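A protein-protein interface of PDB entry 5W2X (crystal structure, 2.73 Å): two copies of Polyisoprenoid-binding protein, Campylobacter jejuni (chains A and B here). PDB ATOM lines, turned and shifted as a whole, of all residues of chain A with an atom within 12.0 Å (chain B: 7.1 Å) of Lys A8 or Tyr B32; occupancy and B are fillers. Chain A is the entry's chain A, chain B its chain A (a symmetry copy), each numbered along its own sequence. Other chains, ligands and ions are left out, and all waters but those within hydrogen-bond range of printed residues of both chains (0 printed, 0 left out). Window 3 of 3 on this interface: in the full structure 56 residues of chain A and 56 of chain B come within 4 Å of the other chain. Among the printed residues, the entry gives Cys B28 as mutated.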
ATOM      1  N   TYR A   4      -8.945  15.363  -7.215  1.00  0.00           N
ATOM      2  CA  TYR A   4      -8.417  14.563  -8.327  1.00  0.00           C
ATOM      3  C   TYR A   4      -8.837  13.106  -8.213  1.00  0.00           C
ATOM      4  O   TYR A   4      -9.305  12.679  -7.154  1.00  0.00           O
ATOM      5  CB  TYR A   4      -6.897  14.688  -8.419  1.00  0.00           C
ATOM      6  CG  TYR A   4      -6.378  16.106  -8.608  1.00  0.00           C
ATOM      7  CD1 TYR A   4      -6.529  17.113  -7.583  1.00  0.00           C
ATOM      8  CD2 TYR A   4      -5.690  16.447  -9.790  1.00  0.00           C
ATOM      9  CE1 TYR A   4      -6.032  18.409  -7.762  1.00  0.00           C
ATOM     10  CE2 TYR A   4      -5.174  17.736  -9.971  1.00  0.00           C
ATOM     11  CZ  TYR A   4      -5.343  18.712  -8.969  1.00  0.00           C
ATOM     12  OH  TYR A   4      -4.815  19.968  -9.210  1.00  0.00           O
ATOM     13  N   THR A   5      -8.684  12.369  -9.308  1.00  0.00           N
ATOM     14  CA  THR A   5      -9.001  10.955  -9.355  1.00  0.00           C
ATOM     15  C   THR A   5      -7.787  10.317  -9.960  1.00  0.00           C
ATOM     16  O   THR A   5      -7.361  10.718 -11.052  1.00  0.00           O
ATOM     17  CB  THR A   5     -10.242  10.665 -10.255  1.00  0.00           C
ATOM     18  OG1 THR A   5     -11.392  11.337  -9.723  1.00  0.00           O
ATOM     19  CG2 THR A   5     -10.551   9.143 -10.365  1.00  0.00           C
ATOM     20  N   LEU A   6      -7.241   9.312  -9.283  1.00  0.00           N
ATOM     21  CA  LEU A   6      -6.094   8.578  -9.844  1.00  0.00           C
ATOM     22  C   LEU A   6      -6.369   8.111 -11.259  1.00  0.00           C
ATOM     23  O   LEU A   6      -7.501   7.786 -11.589  1.00  0.00           O
ATOM     24  CB  LEU A   6      -5.762   7.350  -9.013  1.00  0.00           C
ATOM     25  CG  LEU A   6      -5.519   7.538  -7.534  1.00  0.00           C
ATOM     26  CD1 LEU A   6      -6.750   7.125  -6.737  1.00  0.00           C
ATOM     27  CD2 LEU A   6      -4.350   6.642  -7.256  1.00  0.00           C
ATOM     28  N   ASP A   7      -5.346   8.122 -12.099  1.00  0.00           N
ATOM     29  CA  ASP A   7      -5.385   7.406 -13.360  1.00  0.00           C
ATOM     30  C   ASP A   7      -4.654   6.114 -13.033  1.00  0.00           C
ATOM     31  O   ASP A   7      -3.423   6.081 -13.008  1.00  0.00           O
ATOM     32  CB  ASP A   7      -4.724   8.228 -14.497  1.00  0.00           C
ATOM     33  CG  ASP A   7      -4.357   7.383 -15.758  1.00  0.00           C
ATOM     34  OD1 ASP A   7      -4.841   6.225 -15.911  1.00  0.00           O
ATOM     35  OD2 ASP A   7      -3.571   7.898 -16.605  1.00  0.00           O
ATOM     36  N   LYS A   8      -5.424   5.059 -12.758  1.00  0.00           N
ATOM     37  CA  LYS A   8      -4.875   3.753 -12.354  1.00  0.00           C
ATOM     38  C   LYS A   8      -3.867   3.180 -13.370  1.00  0.00           C
ATOM     39  O   LYS A   8      -2.961   2.418 -12.988  1.00  0.00           O
ATOM     40  CB  LYS A   8      -5.993   2.734 -12.041  1.00  0.00           C
ATOM     41  CG  LYS A   8      -6.753   2.920 -10.717  1.00  0.00           C
ATOM     42  CD  LYS A   8      -7.024   1.567 -10.033  1.00  0.00           C
ATOM     43  CE  LYS A   8      -8.420   1.412  -9.423  1.00  0.00           C
ATOM     44  NZ  LYS A   8      -8.754   2.391  -8.349  1.00  0.00           N
ATOM     45  N   ALA A   9      -4.008   3.576 -14.640  1.00  0.00           N
ATOM     46  CA  ALA A   9      -3.145   3.092 -15.729  1.00  0.00           C
ATOM     47  C   ALA A   9      -1.703   3.627 -15.671  1.00  0.00           C
ATOM     48  O   ALA A   9      -0.773   2.935 -16.075  1.00  0.00           O
ATOM     49  CB  ALA A   9      -3.780   3.389 -17.081  1.00  0.00           C
ATOM     50  N   HIS A  10      -1.523   4.852 -15.169  1.00  0.00           N
ATOM     51  CA  HIS A  10      -0.184   5.450 -14.996  1.00  0.00           C
ATOM     52  C   HIS A  10       0.159   5.746 -13.522  1.00  0.00           C
ATOM     53  O   HIS A  10       0.918   6.670 -13.214  1.00  0.00           O
ATOM     54  CB  HIS A  10      -0.046   6.698 -15.871  1.00  0.00           C
ATOM     55  CG  HIS A  10      -0.225   6.422 -17.325  1.00  0.00           C
ATOM     56  ND1 HIS A  10      -1.427   6.617 -17.976  1.00  0.00           N
ATOM     57  CD2 HIS A  10       0.636   5.932 -18.250  1.00  0.00           C
ATOM     58  CE1 HIS A  10      -1.294   6.277 -19.245  1.00  0.00           C
ATOM     59  NE2 HIS A  10      -0.053   5.858 -19.437  1.00  0.00           N
ATOM     60  N   THR A  11      -0.431   4.955 -12.628  1.00  0.00           N
ATOM     61  CA  THR A  11      -0.148   4.979 -11.198  1.00  0.00           C
ATOM     62  C   THR A  11       0.389   3.597 -10.803  1.00  0.00           C
ATOM     63  O   THR A  11      -0.121   2.567 -11.257  1.00  0.00           O
ATOM     64  CB  THR A  11      -1.398   5.393 -10.366  1.00  0.00           C
ATOM     65  OG1 THR A  11      -1.642   6.801 -10.503  1.00  0.00           O
ATOM     66  CG2 THR A  11      -1.224   5.092  -8.895  1.00  0.00           C
ATOM     67  N   ASP A  12       1.441   3.600  -9.987  1.00  0.00           N
ATOM     68  CA  ASP A  12       2.028   2.393  -9.447  1.00  0.00           C
ATOM     69  C   ASP A  12       2.152   2.509  -7.903  1.00  0.00           C
ATOM     70  O   ASP A  12       2.935   3.324  -7.395  1.00  0.00           O
ATOM     71  CB  ASP A  12       3.375   2.128 -10.134  1.00  0.00           C
ATOM     72  CG  ASP A  12       4.099   0.901  -9.565  1.00  0.00           C
ATOM     73  OD1 ASP A  12       3.745  -0.235  -9.961  1.00  0.00           O
ATOM     74  OD2 ASP A  12       5.018   1.061  -8.717  1.00  0.00           O
ATOM     75  N   VAL A  13       1.378   1.712  -7.158  1.00  0.00           N
ATOM     76  CA  VAL A  13       1.460   1.763  -5.690  1.00  0.00           C
ATOM     77  C   VAL A  13       2.463   0.710  -5.272  1.00  0.00           C
ATOM     78  O   VAL A  13       2.095  -0.439  -5.040  1.00  0.00           O
ATOM     79  CB  VAL A  13       0.065   1.591  -5.033  1.00  0.00           C
ATOM     80  CG1 VAL A  13       0.125   1.647  -3.513  1.00  0.00           C
ATOM     81  CG2 VAL A  13      -0.891   2.662  -5.544  1.00  0.00           C
ATOM     82  N   GLY A  14       3.737   1.106  -5.203  1.00  0.00           N
ATOM     83  CA  GLY A  14       4.866   0.156  -5.153  1.00  0.00           C
ATOM     84  C   GLY A  14       5.732   0.113  -3.903  1.00  0.00           C
ATOM     85  O   GLY A  14       5.758   1.067  -3.120  1.00  0.00           O
ATOM     86  N   PHE A  15       6.453  -1.003  -3.735  1.00  0.00           N
ATOM     87  CA  PHE A  15       7.376  -1.236  -2.602  1.00  0.00           C
ATOM     88  C   PHE A  15       8.567  -2.078  -3.047  1.00  0.00           C
ATOM     89  O   PHE A  15       8.487  -2.739  -4.077  1.00  0.00           O
ATOM     90  CB  PHE A  15       6.660  -1.927  -1.445  1.00  0.00           C
ATOM     91  CG  PHE A  15       6.110  -3.274  -1.800  1.00  0.00           C
ATOM     92  CD1 PHE A  15       4.910  -3.391  -2.490  1.00  0.00           C
ATOM     93  CD2 PHE A  15       6.799  -4.426  -1.458  1.00  0.00           C
ATOM     94  CE1 PHE A  15       4.404  -4.630  -2.833  1.00  0.00           C
ATOM     95  CE2 PHE A  15       6.298  -5.663  -1.795  1.00  0.00           C
ATOM     96  CZ  PHE A  15       5.101  -5.765  -2.482  1.00  0.00           C
ATOM     97  N   CYS B  28       3.971  -4.228  -6.454  1.00  0.00           N
ATOM     98  CA  CYS B  28       2.891  -3.218  -6.370  1.00  0.00           C
ATOM     99  C   CYS B  28       1.576  -3.828  -5.908  1.00  0.00           C
ATOM    100  O   CYS B  28       1.482  -5.034  -5.651  1.00  0.00           O
ATOM    101  CB  CYS B  28       2.658  -2.523  -7.710  1.00  0.00           C
ATOM    102  SG  CYS B  28       2.419  -3.687  -9.055  1.00  0.00           S
ATOM    103  N   PHE B  29       0.562  -2.983  -5.789  1.00  0.00           N
ATOM    104  CA  PHE B  29      -0.780  -3.475  -5.579  1.00  0.00           C
ATOM    105  C   PHE B  29      -1.608  -3.054  -6.780  1.00  0.00           C
ATOM    106  O   PHE B  29      -1.607  -1.867  -7.156  1.00  0.00           O
ATOM    107  CB  PHE B  29      -1.359  -2.951  -4.277  1.00  0.00           C
ATOM    108  CG  PHE B  29      -0.624  -3.418  -3.052  1.00  0.00           C
ATOM    109  CD1 PHE B  29       0.473  -2.703  -2.558  1.00  0.00           C
ATOM    110  CD2 PHE B  29      -1.038  -4.556  -2.366  1.00  0.00           C
ATOM    111  CE1 PHE B  29       1.144  -3.121  -1.408  1.00  0.00           C
ATOM    112  CE2 PHE B  29      -0.365  -4.976  -1.218  1.00  0.00           C
ATOM    113  CZ  PHE B  29       0.729  -4.261  -0.743  1.00  0.00           C
ATOM    114  N   LYS B  30      -2.268  -4.043  -7.396  1.00  0.00           N
ATOM    115  CA  LYS B  30      -3.080  -3.836  -8.591  1.00  0.00           C
ATOM    116  C   LYS B  30      -4.412  -3.113  -8.249  1.00  0.00           C
ATOM    117  O   LYS B  30      -4.932  -2.353  -9.073  1.00  0.00           O
ATOM    118  CB  LYS B  30      -3.271  -5.155  -9.363  1.00  0.00           C
ATOM    119  N   ASP B  31      -4.919  -3.275  -7.022  1.00  0.00           N
ATOM    120  CA  ASP B  31      -6.215  -2.675  -6.644  1.00  0.00           C
ATOM    121  C   ASP B  31      -6.263  -1.823  -5.348  1.00  0.00           C
ATOM    122  O   ASP B  31      -6.057  -2.332  -4.234  1.00  0.00           O
ATOM    123  CB  ASP B  31      -7.288  -3.774  -6.615  1.00  0.00           C
ATOM    124  CG  ASP B  31      -8.683  -3.217  -6.574  1.00  0.00           C
ATOM    125  OD1 ASP B  31      -8.957  -2.208  -7.284  1.00  0.00           O
ATOM    126  OD2 ASP B  31      -9.495  -3.805  -5.827  1.00  0.00           O
ATOM    127  N   TYR B  32      -6.584  -0.540  -5.511  1.00  0.00           N
ATOM    128  CA  TYR B  32      -6.525   0.459  -4.425  1.00  0.00           C
ATOM    129  C   TYR B  32      -7.493   1.576  -4.745  1.00  0.00           C
ATOM    130  O   TYR B  32      -7.846   1.780  -5.904  1.00  0.00           O
ATOM    131  CB  TYR B  32      -5.105   1.072  -4.322  1.00  0.00           C
ATOM    132  CG  TYR B  32      -4.519   1.497  -5.689  1.00  0.00           C
ATOM    133  CD1 TYR B  32      -3.858   0.565  -6.497  1.00  0.00           C
ATOM    134  CD2 TYR B  32      -4.645   2.812  -6.180  1.00  0.00           C
ATOM    135  CE1 TYR B  32      -3.342   0.908  -7.740  1.00  0.00           C
ATOM    136  CE2 TYR B  32      -4.141   3.159  -7.436  1.00  0.00           C
ATOM    137  CZ  TYR B  32      -3.483   2.199  -8.210  1.00  0.00           C
ATOM    138  OH  TYR B  32      -2.947   2.463  -9.463  1.00  0.00           O
ATOM    139  N   SER B  33      -7.908   2.332  -3.747  1.00  0.00           N
ATOM    140  CA  SER B  33      -8.631   3.577  -4.025  1.00  0.00           C
ATOM    141  C   SER B  33      -7.987   4.739  -3.277  1.00  0.00           C
ATOM    142  O   SER B  33      -7.354   4.544  -2.229  1.00  0.00           O
ATOM    143  CB  SER B  33     -10.115   3.469  -3.648  1.00  0.00           C
ATOM    144  OG  SER B  33     -10.308   3.708  -2.263  1.00  0.00           O
ATOM    145  N   ALA B  34      -8.154   5.945  -3.807  1.00  0.00           N
ATOM    146  CA  ALA B  34      -7.663   7.119  -3.119  1.00  0.00           C
ATOM    147  C   ALA B  34      -8.515   8.324  -3.376  1.00  0.00           C
ATOM    148  O   ALA B  34      -9.141   8.444  -4.432  1.00  0.00           O
ATOM    149  CB  ALA B  34      -6.217   7.413  -3.507  1.00  0.00           C
ATOM    150  N   VAL B  50      -5.750   6.829   1.245  1.00  0.00           N
ATOM    151  CA  VAL B  50      -5.597   5.694   0.322  1.00  0.00           C
ATOM    152  C   VAL B  50      -6.040   4.401   1.031  1.00  0.00           C
ATOM    153  O   VAL B  50      -5.788   4.243   2.231  1.00  0.00           O
ATOM    154  CB  VAL B  50      -4.135   5.554  -0.188  1.00  0.00           C
ATOM    155  CG1 VAL B  50      -4.049   4.536  -1.293  1.00  0.00           C
ATOM    156  CG2 VAL B  50      -3.588   6.865  -0.717  1.00  0.00           C
ATOM    157  N   THR B  51      -6.721   3.510   0.295  1.00  0.00           N
ATOM    158  CA  THR B  51      -7.035   2.141   0.750  1.00  0.00           C
ATOM    159  C   THR B  51      -6.545   1.167  -0.299  1.00  0.00           C
ATOM    160  O   THR B  51      -6.800   1.328  -1.498  1.00  0.00           O
ATOM    161  CB  THR B  51      -8.536   1.920   0.990  1.00  0.00           C
ATOM    162  OG1 THR B  51      -9.004   2.907   1.901  1.00  0.00           O
ATOM    163  CG2 THR B  51      -8.810   0.579   1.627  1.00  0.00           C
ATOM    164  N   ILE B  52      -5.819   0.164   0.171  1.00  0.00           N
ATOM    165  CA  ILE B  52      -5.193  -0.784  -0.707  1.00  0.00           C
ATOM    166  C   ILE B  52      -5.736  -2.132  -0.346  1.00  0.00           C
ATOM    167  O   ILE B  52      -5.730  -2.473   0.839  1.00  0.00           O
ATOM    168  CB  ILE B  52      -3.690  -0.801  -0.470  1.00  0.00           C
ATOM    169  CG1 ILE B  52      -3.118   0.549  -0.834  1.00  0.00           C
ATOM    170  CG2 ILE B  52      -3.054  -1.834  -1.368  1.00  0.00           C
ATOM    171  CD1 ILE B  52      -1.868   0.845  -0.067  1.00  0.00           C
ATOM    172  N   LYS B  53      -6.174  -2.887  -1.363  1.00  0.00           N
ATOM    173  CA  LYS B  53      -6.628  -4.284  -1.184  1.00  0.00           C
ATOM    174  C   LYS B  53      -5.418  -5.217  -1.207  1.00  0.00           C
ATOM    175  O   LYS B  53      -4.816  -5.479  -2.281  1.00  0.00           O
ATOM    176  CB  LYS B  53      -7.704  -4.707  -2.212  1.00  0.00           C
ATOM    177  CG  LYS B  53      -8.917  -3.793  -2.220  1.00  0.00           C
ATOM    178  CD  LYS B  53     -10.235  -4.468  -2.581  1.00  0.00           C
ATOM    179  CE  LYS B  53     -11.421  -3.701  -1.976  1.00  0.00           C
ATOM    180  NZ  LYS B  53     -11.339  -3.564  -0.476  1.00  0.00           N
ATOM    181  N   SER B  56      -4.592  -7.769  -3.762  1.00  0.00           N
ATOM    182  CA  SER B  56      -4.226  -7.427  -5.130  1.00  0.00           C
ATOM    183  C   SER B  56      -2.732  -7.239  -5.313  1.00  0.00           C
ATOM    184  O   SER B  56      -2.290  -6.749  -6.362  1.00  0.00           O
ATOM    185  CB  SER B  56      -4.996  -6.193  -5.618  1.00  0.00           C
ATOM    186  OG  SER B  56      -4.552  -5.002  -4.988  1.00  0.00           O
ATOM    187  N   MET B  82      -5.000  -2.445   3.522  1.00  0.00           N
ATOM    188  CA  MET B  82      -4.164  -1.497   4.255  1.00  0.00           C
ATOM    189  C   MET B  82      -4.515  -0.094   3.804  1.00  0.00           C
ATOM    190  O   MET B  82      -4.919   0.123   2.636  1.00  0.00           O
ATOM    191  CB  MET B  82      -2.657  -1.811   4.196  1.00  0.00           C
ATOM    192  CG  MET B  82      -1.942  -1.366   2.935  1.00  0.00           C
ATOM    193  SD  MET B  82      -0.145  -1.626   2.883  1.00  0.00           S
ATOM    194  CE  MET B  82       0.283  -1.330   4.574  1.00  0.00           C
ATOM    195  N   GLU B 164       3.972   6.145  -7.108  1.00  0.00           N
ATOM    196  CA  GLU B 164       4.070   7.004  -8.276  1.00  0.00           C
ATOM    197  C   GLU B 164       2.647   7.267  -8.767  1.00  0.00           C
ATOM    198  O   GLU B 164       1.931   6.331  -9.080  1.00  0.00           O
ATOM    199  CB  GLU B 164       4.938   6.324  -9.344  1.00  0.00           C
ATOM    200  CG  GLU B 164       5.567   7.260 -10.371  1.00  0.00           C
ATOM    201  CD  GLU B 164       6.671   8.129  -9.793  1.00  0.00           C
ATOM    202  OE1 GLU B 164       7.699   7.573  -9.324  1.00  0.00           O
ATOM    203  OE2 GLU B 164       6.500   9.370  -9.815  1.00  0.00           O
ATOM    204  N   VAL B 165       2.230   8.527  -8.814  1.00  0.00           N
ATOM    205  CA  VAL B 165       0.828   8.870  -9.100  1.00  0.00           C
ATOM    206  C   VAL B 165       0.756   9.817 -10.291  1.00  0.00           C
ATOM    207  O   VAL B 165       1.499  10.803 -10.324  1.00  0.00           O
ATOM    208  CB  VAL B 165       0.157   9.535  -7.860  1.00  0.00           C
ATOM    209  CG1 VAL B 165      -1.234  10.067  -8.156  1.00  0.00           C
ATOM    210  CG2 VAL B 165       0.080   8.550  -6.724  1.00  0.00           C
ATOM    211  N   GLU B 166      -0.083   9.472 -11.279  1.00  0.00           N
ATOM    212  CA  GLU B 166      -0.671  10.432 -12.241  1.00  0.00           C
ATOM    213  C   GLU B 166      -2.167  10.540 -11.876  1.00  0.00           C
ATOM    214  O   GLU B 166      -2.746   9.580 -11.341  1.00  0.00           O
ATOM    215  CB  GLU B 166      -0.440  10.028 -13.707  1.00  0.00           C
ATOM    216  N   ASN B 168      -6.081  13.109 -12.535  1.00  0.00           N
ATOM    217  CA  ASN B 168      -6.860  14.123 -13.247  1.00  0.00           C
ATOM    218  C   ASN B 168      -7.966  14.665 -12.364  1.00  0.00           C
ATOM    219  O   ASN B 168      -8.362  14.025 -11.389  1.00  0.00           O
ATOM    220  CB  ASN B 168      -7.446  13.517 -14.512  1.00  0.00           C
ATOM    221  CG  ASN B 168      -6.386  12.853 -15.389  1.00  0.00           C
ATOM    222  OD1 ASN B 168      -5.639  13.525 -16.113  1.00  0.00           O
ATOM    223  ND2 ASN B 168      -6.312  11.526 -15.325  1.00  0.00           N
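No position is printed for both chains.
The side-chain carboxylate (OD1) of Asp A7 sits at hydrogen-bond distance from the backbone NH (N) of Ala A9 (3.1 Å). OD2 of Asp A7 lies within hydrogen-bond range of ND1 of His A10, at 2.8 Å. The backbone carbonyl oxygen (O) of Asp A7 lies within hydrogen-bond range of the side-chain hydroxyl (OG1) of Thr A11 (3.2 Å).
Among the printed residues, merely in contact across the chains: Tyr A4 with Asn B168, Leu A6 with Tyr B32, Leu A6 with Ala B34, Leu A6 with Glu B166, Asp A7 with Asn B168, His A10 with Glu B166, Thr A11 with Glu B164, Thr A11 with Val B165, Asp A12 with Cys B28, Val A13 with Cys B28, Val A13 with Tyr B32, Phe A15 with Cys B28 and Phe A15 with Phe B29.
Printed residues of chain B within 4 Å of Asp A7: Glu B166 (3.1 Å) and Asn B168 (3.8 Å). Of chain B, only Tyr B32 comes within 4 Å of Lys A8. Of the printed residues of chain B, Thr A11 touches Tyr B32, Glu B164, Val B165 and Glu B166. Of the printed residues of chain B, Val A13 touches Cys B28 (3.2 Å), Phe B29 (3.1 Å) and Tyr B32 (3.7 Å). Gly A14 touches none of the printed residues of chain B. No residue of chain A comes within 4 Å of Lys B30. No residue of chain A comes within 4 Å of Asp B31. Tyr B32 touches just these residues of chain A: Leu A6 (3.5 Å), Lys A8 (2.7 Å), Thr A11 (3.2 Å) and Val A13 (3.7 Å). No residue of chain A comes within 4 Å of Ser B33. No residue of chain A comes within 4 Å of Ser B56. Of the printed residues of chain A, Val B165 touches Thr A11 (3.5 Å). Glu B166 touches just these residues of chain A: Leu A6 (3.8 Å), Asp A7 (3.1 Å), His A10 (3.5 Å) and Thr A11 (3.1 Å). The nearest residue of chain B that does not touch Lys A8 is Asp B31 (4.2 Å). The nearest residue of chain A that does not touch Tyr B32 is Asp A12 (4.6 Å). The nearest printed residue of chain B that does not touch Asp A12 is Tyr B32 (4.6 Å).
O of Asn B168 lies within hydrogen-bond range of N of Thr A5, 2.7 Å away. The backbone NH of Asp A7 sits at hydrogen-bond distance from the backbone carbonyl oxygen of Glu B166 (3.1 Å). The side-chain amino group of Lys A8 lies within hydrogen-bond range of the backbone carbonyl oxygen of Tyr B32 (2.7 Å). The backbone carbonyl oxygen of Thr A11 sits close to the side-chain hydroxyl of Tyr B32, at 3.3 Å. The backbone carbonyl oxygen of Glu B166 is in hydrogen-bond range of the side-chain hydroxyl of Thr A11, 3.1 Å away. The backbone NH of Asp A12 lies within hydrogen-bond range of the backbone carbonyl oxygen of Glu B164 (2.9 Å). O of Val A13 lies within hydrogen-bond range of N of Phe B29, at 3.1 Å.
Printed residues of chain B that touch a printed residue of chain A: Cys B28, Phe B29, Tyr B32, Ala B34, Glu B164, Val B165, Glu B166 and Asn B168. Hydrophobic or aromatic side chains of chain B that line the printed part of chain A: Phe B29, Tyr B32 and Ala B34. Printed residues of chain A that touch a printed residue of chain B: Tyr A4, Thr A5, Leu A6, Asp A7, Lys A8, His A10, Thr A11, Asp A12, Val A13 and Phe A15. Hydrophobic or aromatic side chains of chain A within 4 Å of the printed part of chain B: Tyr A4, Leu A6, His A10, Val A13 and Phe A15. Among the printed residues, no Asp or Glu carboxylate lies within 4 Å of a Lys or Arg side-chain nitrogen of the other chain.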
